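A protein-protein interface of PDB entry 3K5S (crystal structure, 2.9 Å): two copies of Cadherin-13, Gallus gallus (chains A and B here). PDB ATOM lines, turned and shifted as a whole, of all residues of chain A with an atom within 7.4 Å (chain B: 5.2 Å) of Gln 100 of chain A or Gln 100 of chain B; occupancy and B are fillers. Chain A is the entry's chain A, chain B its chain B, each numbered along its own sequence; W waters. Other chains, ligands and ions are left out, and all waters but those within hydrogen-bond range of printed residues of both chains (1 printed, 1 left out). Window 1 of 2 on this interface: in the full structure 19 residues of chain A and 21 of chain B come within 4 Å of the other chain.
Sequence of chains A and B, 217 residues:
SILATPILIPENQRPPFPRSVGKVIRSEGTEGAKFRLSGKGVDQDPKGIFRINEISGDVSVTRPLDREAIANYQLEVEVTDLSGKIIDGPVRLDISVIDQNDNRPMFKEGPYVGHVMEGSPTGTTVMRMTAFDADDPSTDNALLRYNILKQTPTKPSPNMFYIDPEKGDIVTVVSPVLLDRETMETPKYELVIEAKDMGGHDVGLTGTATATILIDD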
ATOM      1  N   PRO A  10      -9.581 -12.781  19.859  1.00  0.00           N
ATOM      2  CA  PRO A  10     -10.987 -12.556  20.208  1.00  0.00           C
ATOM      3  C   PRO A  10     -11.085 -11.685  21.446  1.00  0.00           C
ATOM      4  O   PRO A  10     -10.334 -11.917  22.388  1.00  0.00           O
ATOM      5  CB  PRO A  10     -11.497 -13.969  20.555  1.00  0.00           C
ATOM      6  CG  PRO A  10     -10.380 -14.929  20.203  1.00  0.00           C
ATOM      7  CD  PRO A  10      -9.118 -14.125  20.252  1.00  0.00           C
ATOM      8  N   GLU A  11     -11.997 -10.723  21.475  1.00  0.00           N
ATOM      9  CA  GLU A  11     -12.195  -9.949  22.701  1.00  0.00           C
ATOM     10  C   GLU A  11     -12.729 -10.820  23.843  1.00  0.00           C
ATOM     11  O   GLU A  11     -13.053 -11.996  23.645  1.00  0.00           O
ATOM     12  CB  GLU A  11     -13.142  -8.791  22.450  1.00  0.00           C
ATOM     13  CG  GLU A  11     -14.421  -9.245  21.806  1.00  0.00           C
ATOM     14  CD  GLU A  11     -15.516  -8.233  21.926  1.00  0.00           C
ATOM     15  OE1 GLU A  11     -16.481  -8.329  21.158  1.00  0.00           O
ATOM     16  OE2 GLU A  11     -15.409  -7.340  22.782  1.00  0.00           O
ATOM     17  N   ASN A  12     -12.827 -10.235  25.035  1.00  0.00           N
ATOM     18  CA  ASN A  12     -13.236 -10.965  26.236  1.00  0.00           C
ATOM     19  C   ASN A  12     -12.627 -12.368  26.355  1.00  0.00           C
ATOM     20  O   ASN A  12     -13.342 -13.348  26.610  1.00  0.00           O
ATOM     21  CB  ASN A  12     -14.759 -11.089  26.322  1.00  0.00           C
ATOM     22  CG  ASN A  12     -15.475  -9.798  26.015  1.00  0.00           C
ATOM     23  OD1 ASN A  12     -15.093  -8.720  26.477  1.00  0.00           O
ATOM     24  ND2 ASN A  12     -16.536  -9.902  25.230  1.00  0.00           N
ATOM     25  N   GLN A  13     -11.320 -12.478  26.151  1.00  0.00           N
ATOM     26  CA  GLN A  13     -10.619 -13.715  26.493  1.00  0.00           C
ATOM     27  C   GLN A  13     -10.626 -13.963  28.016  1.00  0.00           C
ATOM     28  O   GLN A  13     -10.807 -13.041  28.824  1.00  0.00           O
ATOM     29  CB  GLN A  13      -9.178 -13.683  25.981  1.00  0.00           C
ATOM     30  CG  GLN A  13      -8.941 -14.352  24.649  1.00  0.00           C
ATOM     31  CD  GLN A  13      -7.462 -14.393  24.308  1.00  0.00           C
ATOM     32  OE1 GLN A  13      -6.694 -13.540  24.757  1.00  0.00           O
ATOM     33  NE2 GLN A  13      -7.054 -15.386  23.519  1.00  0.00           N
ATOM     34  N   ARG A  67     -13.295  -5.117  22.124  1.00  0.00           N
ATOM     35  CA  ARG A  67     -13.355  -4.617  20.756  1.00  0.00           C
ATOM     36  C   ARG A  67     -13.947  -3.213  20.650  1.00  0.00           C
ATOM     37  O   ARG A  67     -13.461  -2.409  19.866  1.00  0.00           O
ATOM     38  CB  ARG A  67     -14.110  -5.575  19.845  1.00  0.00           C
ATOM     39  CG  ARG A  67     -13.951  -5.258  18.372  1.00  0.00           C
ATOM     40  CD  ARG A  67     -15.108  -5.810  17.569  1.00  0.00           C
ATOM     41  NE  ARG A  67     -16.348  -5.077  17.829  1.00  0.00           N
ATOM     42  CZ  ARG A  67     -16.743  -4.028  17.115  1.00  0.00           C
ATOM     43  NH1 ARG A  67     -15.999  -3.605  16.096  1.00  0.00           N
ATOM     44  NH2 ARG A  67     -17.874  -3.407  17.408  1.00  0.00           N
ATOM     45  N   GLU A  68     -14.987  -2.909  21.425  1.00  0.00           N
ATOM     46  CA  GLU A  68     -15.633  -1.600  21.322  1.00  0.00           C
ATOM     47  C   GLU A  68     -14.745  -0.506  21.907  1.00  0.00           C
ATOM     48  O   GLU A  68     -14.934   0.681  21.637  1.00  0.00           O
ATOM     49  CB  GLU A  68     -17.000  -1.560  22.012  1.00  0.00           C
ATOM     50  CG  GLU A  68     -17.627  -2.897  22.382  1.00  0.00           C
ATOM     51  CD  GLU A  68     -17.516  -3.961  21.306  1.00  0.00           C
ATOM     52  OE1 GLU A  68     -18.091  -3.799  20.207  1.00  0.00           O
ATOM     53  OE2 GLU A  68     -16.859  -4.985  21.589  1.00  0.00           O
ATOM     54  N   VAL A  97      -8.980  -7.219  16.525  1.00  0.00           N
ATOM     55  CA  VAL A  97      -9.739  -7.924  17.561  1.00  0.00           C
ATOM     56  C   VAL A  97     -11.099  -8.483  17.076  1.00  0.00           C
ATOM     57  O   VAL A  97     -11.961  -7.749  16.584  1.00  0.00           O
ATOM     58  CB  VAL A  97      -9.881  -7.052  18.830  1.00  0.00           C
ATOM     59  CG1 VAL A  97     -10.155  -7.926  20.032  1.00  0.00           C
ATOM     60  CG2 VAL A  97      -8.595  -6.245  19.053  1.00  0.00           C
ATOM     61  N   ILE A  98     -11.263  -9.798  17.192  1.00  0.00           N
ATOM     62  CA  ILE A  98     -12.488 -10.474  16.755  1.00  0.00           C
ATOM     63  C   ILE A  98     -13.688 -10.086  17.612  1.00  0.00           C
ATOM     64  O   ILE A  98     -13.633 -10.138  18.848  1.00  0.00           O
ATOM     65  CB  ILE A  98     -12.349 -12.009  16.807  1.00  0.00           C
ATOM     66  CG1 ILE A  98     -11.146 -12.478  15.993  1.00  0.00           C
ATOM     67  CG2 ILE A  98     -13.592 -12.661  16.254  1.00  0.00           C
ATOM     68  CD1 ILE A  98     -11.367 -12.319  14.510  1.00  0.00           C
ATOM     69  N   ASP A  99     -14.771  -9.697  16.945  1.00  0.00           N
ATOM     70  CA  ASP A  99     -15.987  -9.287  17.629  1.00  0.00           C
ATOM     71  C   ASP A  99     -16.610 -10.476  18.322  1.00  0.00           C
ATOM     72  O   ASP A  99     -16.637 -11.589  17.791  1.00  0.00           O
ATOM     73  CB  ASP A  99     -16.991  -8.701  16.632  1.00  0.00           C
ATOM     74  CG  ASP A  99     -18.153  -7.998  17.309  1.00  0.00           C
ATOM     75  OD1 ASP A  99     -19.269  -8.036  16.762  1.00  0.00           O
ATOM     76  OD2 ASP A  99     -17.949  -7.388  18.369  1.00  0.00           O
ATOM     77  N   GLN A 100     -17.112 -10.228  19.518  1.00  0.00           N
ATOM     78  CA  GLN A 100     -17.870 -11.218  20.259  1.00  0.00           C
ATOM     79  C   GLN A 100     -19.183 -10.515  20.650  1.00  0.00           C
ATOM     80  O   GLN A 100     -19.185  -9.326  20.937  1.00  0.00           O
ATOM     81  CB  GLN A 100     -17.052 -11.694  21.469  1.00  0.00           C
ATOM     82  CG  GLN A 100     -17.311 -13.138  21.895  1.00  0.00           C
ATOM     83  CD  GLN A 100     -16.566 -14.170  21.061  1.00  0.00           C
ATOM     84  OE1 GLN A 100     -15.527 -14.673  21.476  1.00  0.00           O
ATOM     85  NE2 GLN A 100     -17.101 -14.500  19.891  1.00  0.00           N
ATOM     86  N   ASN A 101     -20.304 -11.220  20.604  1.00  0.00           N
ATOM     87  CA  ASN A 101     -21.600 -10.571  20.795  1.00  0.00           C
ATOM     88  C   ASN A 101     -21.861 -10.127  22.245  1.00  0.00           C
ATOM     89  O   ASN A 101     -22.534 -10.812  22.998  1.00  0.00           O
ATOM     90  CB  ASN A 101     -22.728 -11.478  20.299  1.00  0.00           C
ATOM     91  CG  ASN A 101     -24.027 -10.726  20.079  1.00  0.00           C
ATOM     92  OD1 ASN A 101     -24.019  -9.594  19.608  1.00  0.00           O
ATOM     93  ND2 ASN A 101     -25.152 -11.358  20.407  1.00  0.00           N
ATOM     94  N   ASP A 102     -21.342  -8.969  22.631  1.00  0.00           N
ATOM     95  CA  ASP A 102     -21.443  -8.554  24.021  1.00  0.00           C
ATOM     96  C   ASP A 102     -22.082  -7.199  24.201  1.00  0.00           C
ATOM     97  O   ASP A 102     -21.983  -6.590  25.265  1.00  0.00           O
ATOM     98  CB  ASP A 102     -20.081  -8.616  24.738  1.00  0.00           C
ATOM     99  CG  ASP A 102     -19.023  -7.746  24.083  1.00  0.00           C
ATOM    100  OD1 ASP A 102     -19.366  -6.758  23.399  1.00  0.00           O
ATOM    101  OD2 ASP A 102     -17.828  -8.052  24.262  1.00  0.00           O
ATOM    102  N   ASN A 103     -22.743  -6.720  23.167  1.00  0.00           N
ATOM    103  CA  ASN A 103     -23.511  -5.498  23.316  1.00  0.00           C
ATOM    104  C   ASN A 103     -24.942  -5.743  22.906  1.00  0.00           C
ATOM    105  O   ASN A 103     -25.195  -6.302  21.858  1.00  0.00           O
ATOM    106  CB  ASN A 103     -22.903  -4.367  22.494  1.00  0.00           C
ATOM    107  CG  ASN A 103     -21.742  -3.706  23.193  1.00  0.00           C
ATOM    108  OD1 ASN A 103     -21.928  -2.962  24.157  1.00  0.00           O
ATOM    109  ND2 ASN A 103     -20.532  -3.959  22.702  1.00  0.00           N
ATOM    110  N   ASP A 135     -21.934  -3.585  18.556  1.00  0.00           N
ATOM    111  CA  ASP A 135     -21.076  -4.626  17.992  1.00  0.00           C
ATOM    112  C   ASP A 135     -20.760  -4.434  16.502  1.00  0.00           C
ATOM    113  O   ASP A 135     -20.996  -3.364  15.941  1.00  0.00           O
ATOM    114  CB  ASP A 135     -21.641  -6.017  18.299  1.00  0.00           C
ATOM    115  CG  ASP A 135     -21.594  -6.335  19.791  1.00  0.00           C
ATOM    116  OD1 ASP A 135     -21.106  -5.485  20.564  1.00  0.00           O
ATOM    117  OD2 ASP A 135     -22.033  -7.421  20.208  1.00  0.00           O
ATOM    118  N   ASP A 136     -20.203  -5.460  15.871  1.00  0.00           N
ATOM    119  CA  ASP A 136     -19.668  -5.321  14.521  1.00  0.00           C
ATOM    120  C   ASP A 136     -20.717  -5.654  13.454  1.00  0.00           C
ATOM    121  O   ASP A 136     -21.156  -6.801  13.341  1.00  0.00           O
ATOM    122  CB  ASP A 136     -18.427  -6.204  14.375  1.00  0.00           C
ATOM    123  CG  ASP A 136     -17.787  -6.093  13.012  1.00  0.00           C
ATOM    124  OD1 ASP A 136     -18.467  -5.614  12.079  1.00  0.00           O
ATOM    125  OD2 ASP A 136     -16.606  -6.499  12.880  1.00  0.00           O
ATOM    126  N   THR A 139     -20.633  -8.630  11.119  1.00  0.00           N
ATOM    127  CA  THR A 139     -20.911  -9.940  11.675  1.00  0.00           C
ATOM    128  C   THR A 139     -22.400 -10.046  11.979  1.00  0.00           C
ATOM    129  O   THR A 139     -23.185  -9.199  11.547  1.00  0.00           O
ATOM    130  CB  THR A 139     -20.082 -10.171  12.958  1.00  0.00           C
ATOM    131  OG1 THR A 139     -20.402  -9.173  13.940  1.00  0.00           O
ATOM    132  CG2 THR A 139     -18.596 -10.099  12.643  1.00  0.00           C
ATOM    133  N   ASP A 140     -22.792 -11.087  12.707  1.00  0.00           N
ATOM    134  CA  ASP A 140     -24.181 -11.247  13.128  1.00  0.00           C
ATOM    135  C   ASP A 140     -24.385 -10.572  14.469  1.00  0.00           C
ATOM    136  O   ASP A 140     -25.506 -10.431  14.940  1.00  0.00           O
ATOM    137  CB  ASP A 140     -24.555 -12.725  13.284  1.00  0.00           C
ATOM    138  CG  ASP A 140     -24.596 -13.467  11.969  1.00  0.00           C
ATOM    139  OD1 ASP A 140     -24.596 -12.817  10.903  1.00  0.00           O
ATOM    140  OD2 ASP A 140     -24.632 -14.714  12.002  1.00  0.00           O
ATOM    141  N   ASN A 141     -23.304 -10.159  15.101  1.00  0.00           N
ATOM    142  CA  ASN A 141     -23.431  -9.681  16.455  1.00  0.00           C
ATOM    143  C   ASN A 141     -24.237  -8.392  16.485  1.00  0.00           C
ATOM    144  O   ASN A 141     -25.034  -8.181  17.379  1.00  0.00           O
ATOM    145  CB  ASN A 141     -22.066  -9.592  17.110  1.00  0.00           C
ATOM    146  CG  ASN A 141     -21.338 -10.928  17.096  1.00  0.00           C
ATOM    147  OD1 ASN A 141     -21.914 -11.961  16.753  1.00  0.00           O
ATOM    148  ND2 ASN A 141     -20.064 -10.911  17.466  1.00  0.00           N
ATOM    149  N   MET A 198     -28.185 -11.254  15.767  1.00  0.00           N
ATOM    150  CA  MET A 198     -27.935 -12.521  15.098  1.00  0.00           C
ATOM    151  C   MET A 198     -28.983 -12.791  14.022  1.00  0.00           C
ATOM    152  O   MET A 198     -29.384 -13.936  13.803  1.00  0.00           O
ATOM    153  CB  MET A 198     -27.919 -13.671  16.112  1.00  0.00           C
ATOM    154  CG  MET A 198     -27.110 -13.423  17.392  1.00  0.00           C
ATOM    155  SD  MET A 198     -25.315 -13.759  17.361  1.00  0.00           S
ATOM    156  CE  MET A 198     -25.163 -15.017  16.080  1.00  0.00           C
ATOM    157  N   PRO B  10     -13.620 -16.473  12.819  1.00  0.00           N
ATOM    158  CA  PRO B  10     -14.851 -16.480  13.607  1.00  0.00           C
ATOM    159  C   PRO B  10     -15.854 -17.380  12.910  1.00  0.00           C
ATOM    160  O   PRO B  10     -15.887 -17.401  11.679  1.00  0.00           O
ATOM    161  CB  PRO B  10     -15.342 -15.031  13.515  1.00  0.00           C
ATOM    162  CG  PRO B  10     -14.248 -14.261  12.903  1.00  0.00           C
ATOM    163  CD  PRO B  10     -13.470 -15.222  12.070  1.00  0.00           C
ATOM    164  N   GLU B  11     -16.650 -18.123  13.665  1.00  0.00           N
ATOM    165  CA  GLU B  11     -17.716 -18.858  13.030  1.00  0.00           C
ATOM    166  C   GLU B  11     -18.749 -17.857  12.541  1.00  0.00           C
ATOM    167  O   GLU B  11     -18.653 -16.653  12.831  1.00  0.00           O
ATOM    168  CB  GLU B  11     -18.346 -19.877  13.978  1.00  0.00           C
ATOM    169  CG  GLU B  11     -18.771 -19.340  15.330  1.00  0.00           C
ATOM    170  CD  GLU B  11     -19.563 -20.362  16.125  1.00  0.00           C
ATOM    171  OE1 GLU B  11     -19.787 -20.141  17.325  1.00  0.00           O
ATOM    172  OE2 GLU B  11     -19.969 -21.391  15.545  1.00  0.00           O
ATOM    173  N   ASN B  12     -19.706 -18.362  11.769  1.00  0.00           N
ATOM    174  CA  ASN B  12     -20.875 -17.600  11.353  1.00  0.00           C
ATOM    175  C   ASN B  12     -20.556 -16.309  10.607  1.00  0.00           C
ATOM    176  O   ASN B  12     -21.300 -15.330  10.718  1.00  0.00           O
ATOM    177  CB  ASN B  12     -21.768 -17.267  12.559  1.00  0.00           C
ATOM    178  CG  ASN B  12     -22.116 -18.483  13.402  1.00  0.00           C
ATOM    179  OD1 ASN B  12     -22.322 -19.592  12.892  1.00  0.00           O
ATOM    180  ND2 ASN B  12     -22.210 -18.268  14.707  1.00  0.00           N
ATOM    181  N   GLU B  68     -19.090 -25.595  16.897  1.00  0.00           N
ATOM    182  CA  GLU B  68     -19.559 -26.787  17.610  1.00  0.00           C
ATOM    183  C   GLU B  68     -19.861 -27.960  16.689  1.00  0.00           C
ATOM    184  O   GLU B  68     -20.175 -29.051  17.151  1.00  0.00           O
ATOM    185  CB  GLU B  68     -20.741 -26.485  18.515  1.00  0.00           C
ATOM    186  CG  GLU B  68     -21.491 -25.264  18.107  1.00  0.00           C
ATOM    187  CD  GLU B  68     -20.941 -23.990  18.729  1.00  0.00           C
ATOM    188  OE1 GLU B  68     -19.950 -24.033  19.494  1.00  0.00           O
ATOM    189  OE2 GLU B  68     -21.527 -22.931  18.450  1.00  0.00           O
ATOM    190  N   ILE B  98     -13.127 -19.697  15.796  1.00  0.00           N
ATOM    191  CA  ILE B  98     -13.328 -18.929  17.013  1.00  0.00           C
ATOM    192  C   ILE B  98     -14.777 -18.985  17.476  1.00  0.00           C
ATOM    193  O   ILE B  98     -15.705 -18.757  16.697  1.00  0.00           O
ATOM    194  CB  ILE B  98     -12.944 -17.459  16.795  1.00  0.00           C
ATOM    195  CG1 ILE B  98     -11.587 -17.362  16.096  1.00  0.00           C
ATOM    196  CG2 ILE B  98     -12.928 -16.719  18.124  1.00  0.00           C
ATOM    197  CD1 ILE B  98     -10.445 -17.960  16.908  1.00  0.00           C
ATOM    198  N   ASP B  99     -14.970 -19.287  18.749  1.00  0.00           N
ATOM    199  CA  ASP B  99     -16.312 -19.332  19.290  1.00  0.00           C
ATOM    200  C   ASP B  99     -17.033 -18.006  19.074  1.00  0.00           C
ATOM    201  O   ASP B  99     -16.457 -16.918  19.242  1.00  0.00           O
ATOM    202  CB  ASP B  99     -16.286 -19.668  20.785  1.00  0.00           C
ATOM    203  CG  ASP B  99     -17.577 -20.315  21.257  1.00  0.00           C
ATOM    204  OD1 ASP B  99     -18.188 -19.811  22.227  1.00  0.00           O
ATOM    205  OD2 ASP B  99     -17.971 -21.327  20.641  1.00  0.00           O
ATOM    206  N   GLN B 100     -18.298 -18.121  18.681  1.00  0.00           N
ATOM    207  CA  GLN B 100     -19.242 -17.015  18.702  1.00  0.00           C
ATOM    208  C   GLN B 100     -20.333 -17.454  19.668  1.00  0.00           C
ATOM    209  O   GLN B 100     -20.511 -18.638  19.885  1.00  0.00           O
ATOM    210  CB  GLN B 100     -19.800 -16.770  17.301  1.00  0.00           C
ATOM    211  CG  GLN B 100     -19.848 -15.308  16.916  1.00  0.00           C
ATOM    212  CD  GLN B 100     -18.499 -14.631  17.069  1.00  0.00           C
ATOM    213  OE1 GLN B 100     -17.456 -15.291  17.099  1.00  0.00           O
ATOM    214  NE2 GLN B 100     -18.509 -13.306  17.171  1.00  0.00           N
ATOM    215  N   ASN B 101     -21.049 -16.528  20.282  1.00  0.00           N
ATOM    216  CA  ASN B 101     -22.032 -16.937  21.281  1.00  0.00           C
ATOM    217  C   ASN B 101     -23.392 -17.236  20.669  1.00  0.00           C
ATOM    218  O   ASN B 101     -24.302 -16.419  20.735  1.00  0.00           O
ATOM    219  CB  ASN B 101     -22.175 -15.888  22.372  1.00  0.00           C
ATOM    220  CG  ASN B 101     -23.069 -16.350  23.487  1.00  0.00           C
ATOM    221  OD1 ASN B 101     -23.542 -17.481  23.470  1.00  0.00           O
ATOM    222  ND2 ASN B 101     -23.314 -15.482  24.463  1.00  0.00           N
ATOM    223  N   ASP B 102     -23.533 -18.417  20.077  1.00  0.00           N
ATOM    224  CA  ASP B 102     -24.750 -18.747  19.337  1.00  0.00           C
ATOM    225  C   ASP B 102     -25.479 -19.958  19.888  1.00  0.00           C
ATOM    226  O   ASP B 102     -26.216 -20.630  19.178  1.00  0.00           O
ATOM    227  CB  ASP B 102     -24.459 -18.916  17.842  1.00  0.00           C
ATOM    228  CG  ASP B 102     -23.344 -19.890  17.572  1.00  0.00           C
ATOM    229  OD1 ASP B 102     -22.668 -20.306  18.539  1.00  0.00           O
ATOM    230  OD2 ASP B 102     -23.140 -20.237  16.389  1.00  0.00           O
ATOM    231  N   ASN B 103     -25.264 -20.221  21.166  1.00  0.00           N
ATOM    232  CA  ASN B 103     -26.024 -21.239  21.862  1.00  0.00           C
ATOM    233  C   ASN B 103     -26.594 -20.684  23.160  1.00  0.00           C
ATOM    234  O   ASN B 103     -25.910 -19.970  23.887  1.00  0.00           O
ATOM    235  CB  ASN B 103     -25.167 -22.484  22.113  1.00  0.00           C
ATOM    236  CG  ASN B 103     -24.939 -23.299  20.845  1.00  0.00           C
ATOM    237  OD1 ASN B 103     -25.663 -24.263  20.567  1.00  0.00           O
ATOM    238  ND2 ASN B 103     -23.942 -22.905  20.059  1.00  0.00           N
ATOM    239  N   ASP B 135     -21.480 -23.926  23.521  1.00  0.00           N
ATOM    240  CA  ASP B 135     -20.391 -23.034  23.143  1.00  0.00           C
ATOM    241  C   ASP B 135     -19.123 -23.446  23.855  1.00  0.00           C
ATOM    242  O   ASP B 135     -19.145 -24.350  24.680  1.00  0.00           O
ATOM    243  CB  ASP B 135     -20.723 -21.587  23.504  1.00  0.00           C
ATOM    244  CG  ASP B 135     -21.861 -21.031  22.678  1.00  0.00           C
ATOM    245  OD1 ASP B 135     -21.943 -21.357  21.479  1.00  0.00           O
ATOM    246  OD2 ASP B 135     -22.685 -20.270  23.218  1.00  0.00           O
ATOM    247  N   THR B 139     -14.388 -20.050  27.187  1.00  0.00           N
ATOM    248  CA  THR B 139     -14.673 -18.664  26.857  1.00  0.00           C
ATOM    249  C   THR B 139     -15.846 -18.204  27.694  1.00  0.00           C
ATOM    250  O   THR B 139     -16.598 -19.033  28.178  1.00  0.00           O
ATOM    251  CB  THR B 139     -15.093 -18.539  25.397  1.00  0.00           C
ATOM    252  OG1 THR B 139     -14.284 -19.406  24.597  1.00  0.00           O
ATOM    253  CG2 THR B 139     -14.939 -17.107  24.931  1.00  0.00           C
ATOM    254  N   ASN B 141     -18.384 -17.279  26.520  1.00  0.00           N
ATOM    255  CA  ASN B 141     -19.549 -17.739  25.754  1.00  0.00           C
ATOM    256  C   ASN B 141     -20.214 -19.021  26.271  1.00  0.00           C
ATOM    257  O   ASN B 141     -21.306 -19.353  25.854  1.00  0.00           O
ATOM    258  CB  ASN B 141     -19.211 -17.889  24.265  1.00  0.00           C
ATOM    259  CG  ASN B 141     -18.881 -16.560  23.594  1.00  0.00           C
ATOM    260  OD1 ASN B 141     -19.054 -15.472  24.172  1.00  0.00           O
ATOM    261  ND2 ASN B 141     -18.398 -16.642  22.363  1.00  0.00           N
HETATM  262  O   HOH W   1     -21.322 -13.264  12.076  1.00  0.00           O
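The side-chain carboxylate (OD1) of Asp 99 of chain A lies within hydrogen-bond range of the backbone NH (N) of Asp 136 of chain A. O of Asp 140 of chain A sits at hydrogen-bond distance from N of Met 198 of chain A (2.9 Å). NE of Arg 67 of chain A lies close to OD2 of Asp 99 of chain A (2.9 Å). OD2 of Asp 102 of chain B sits close to ND2 of Asn 12 of chain B (2.8 Å). OD1 of Asp 99 of chain B lies close to ND2 of Asn 141 of chain B (3.2 Å). The side-chain carboxylate (OD1) of Asp 99 of chain A sits at hydrogen-bond distance from the side-chain amide nitrogen (ND2) of Asn 141 of chain A, at 3.1 Å.
Ile 98 of chain B touches Pro 10 of chain A (CG2 to CG, 3.7 Å). Ile 98 of chain A touches Pro 10 of chain B. ND2 of Asn 141 of chain B touches CD of Gln 100 of chain A, 3.3 Å away. Asp 140 of chain A touches Asn 12 of chain B (OD2 to O, 3.6 Å).
Pro 10 of chain A touches Ile 98 of chain B, and with the chains exchanged Ile 98 of chain A touches Pro 10 of chain B. Asp 99 of chain A touches Gln 100 of chain B, and with the chains exchanged Gln 100 of chain A touches Asp 99 of chain B. Gln 100 of chain B touches its own counterpart, Gln 100 of chain A. Gln 100 of chain A touches Asn 141 of chain B, and with the chains exchanged Asn 141 of chain A touches Gln 100 of chain B. Positions printed for both chains: 10, 11, 12, 68, 98, 99, 100, 101, 102, 103, 135, 139 and 141. Of the 8 pairs that touch across the chains among the printed residues, 7 have their exchanged pair printed and touching as well.
Of the 13 printed residues of chain B, 6 touch a printed residue of chain A. Hydrophobic or aromatic side chains of chain B within 4 Å of the printed part of chain A: Pro 10 and Ile 98. Printed residues of chain A that touch a printed residue of chain B: Pro 10, Ile 98, Asp 99, Gln 100, Asp 140 and Asn 141. Among the printed residues, 8 pairs touch across the chains. Among the printed residues, no Asp or Glu carboxylate lies within 4 Å of a Lys or Arg side-chain nitrogen of the other chain.
Of chain B, only Asp 99 (2.6 Å), Gln 100 (2.9 Å) and Asn 141 (3.3 Å) come within 4 Å of Gln 100 of chain A. Of the printed residues of chain B, Asp 140 of chain A touches Asn 12. Of the printed residues of chain A, Asn 141 of chain B touches Gln 100 (3.3 Å). Printed residues of chain B within 4 Å of Asp 99 of chain A: Gln 100 (2.6 Å). Of the printed residues of chain A, Asn 12 of chain B touches Asp 140. Printed residues of chain B within 4 Å of Ile 98 of chain A: Pro 10 (3.8 Å). Glu 68 of chain A touches none of the printed residues of chain B. Val 97 of chain A touches none of the printed residues of chain B. The nearest residue of chain B that does not touch Gln 100 of chain A is Thr 139 of chain B (4.3 Å). The nearest residue of chain A that does not touch Gln 100 of chain B is Asn 101 of chain A (4.4 Å). The nearest printed residue of chain A that does not touch Pro 10 of chain B is Asp 99 of chain A (5.6 Å).
The side-chain amide nitrogen (NE2) of Gln 100 of chain B lies close to the side-chain amide nitrogen (ND2) of Asn 141 of chain A, 2.9 Å away. NE2 of Gln 100 of chain A sits at hydrogen-bond distance from OE1 of Gln 100 of chain B, at 2.9 Å. The backbone carbonyl oxygen of Asp 99 of chain B is in hydrogen-bond range of the side-chain amide nitrogen of Gln 100 of chain A (2.6 Å). The backbone carbonyl oxygen (O) of Asp 99 of chain A lies within hydrogen-bond range of the side-chain amide nitrogen (NE2) of Gln 100 of chain B (2.6 Å).
Water W1 bridges the backbone carbonyl oxygen of Asn 12 of chain B (2.5 Å) and the backbone NH of Asp 140 of chain A (2.7 Å).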
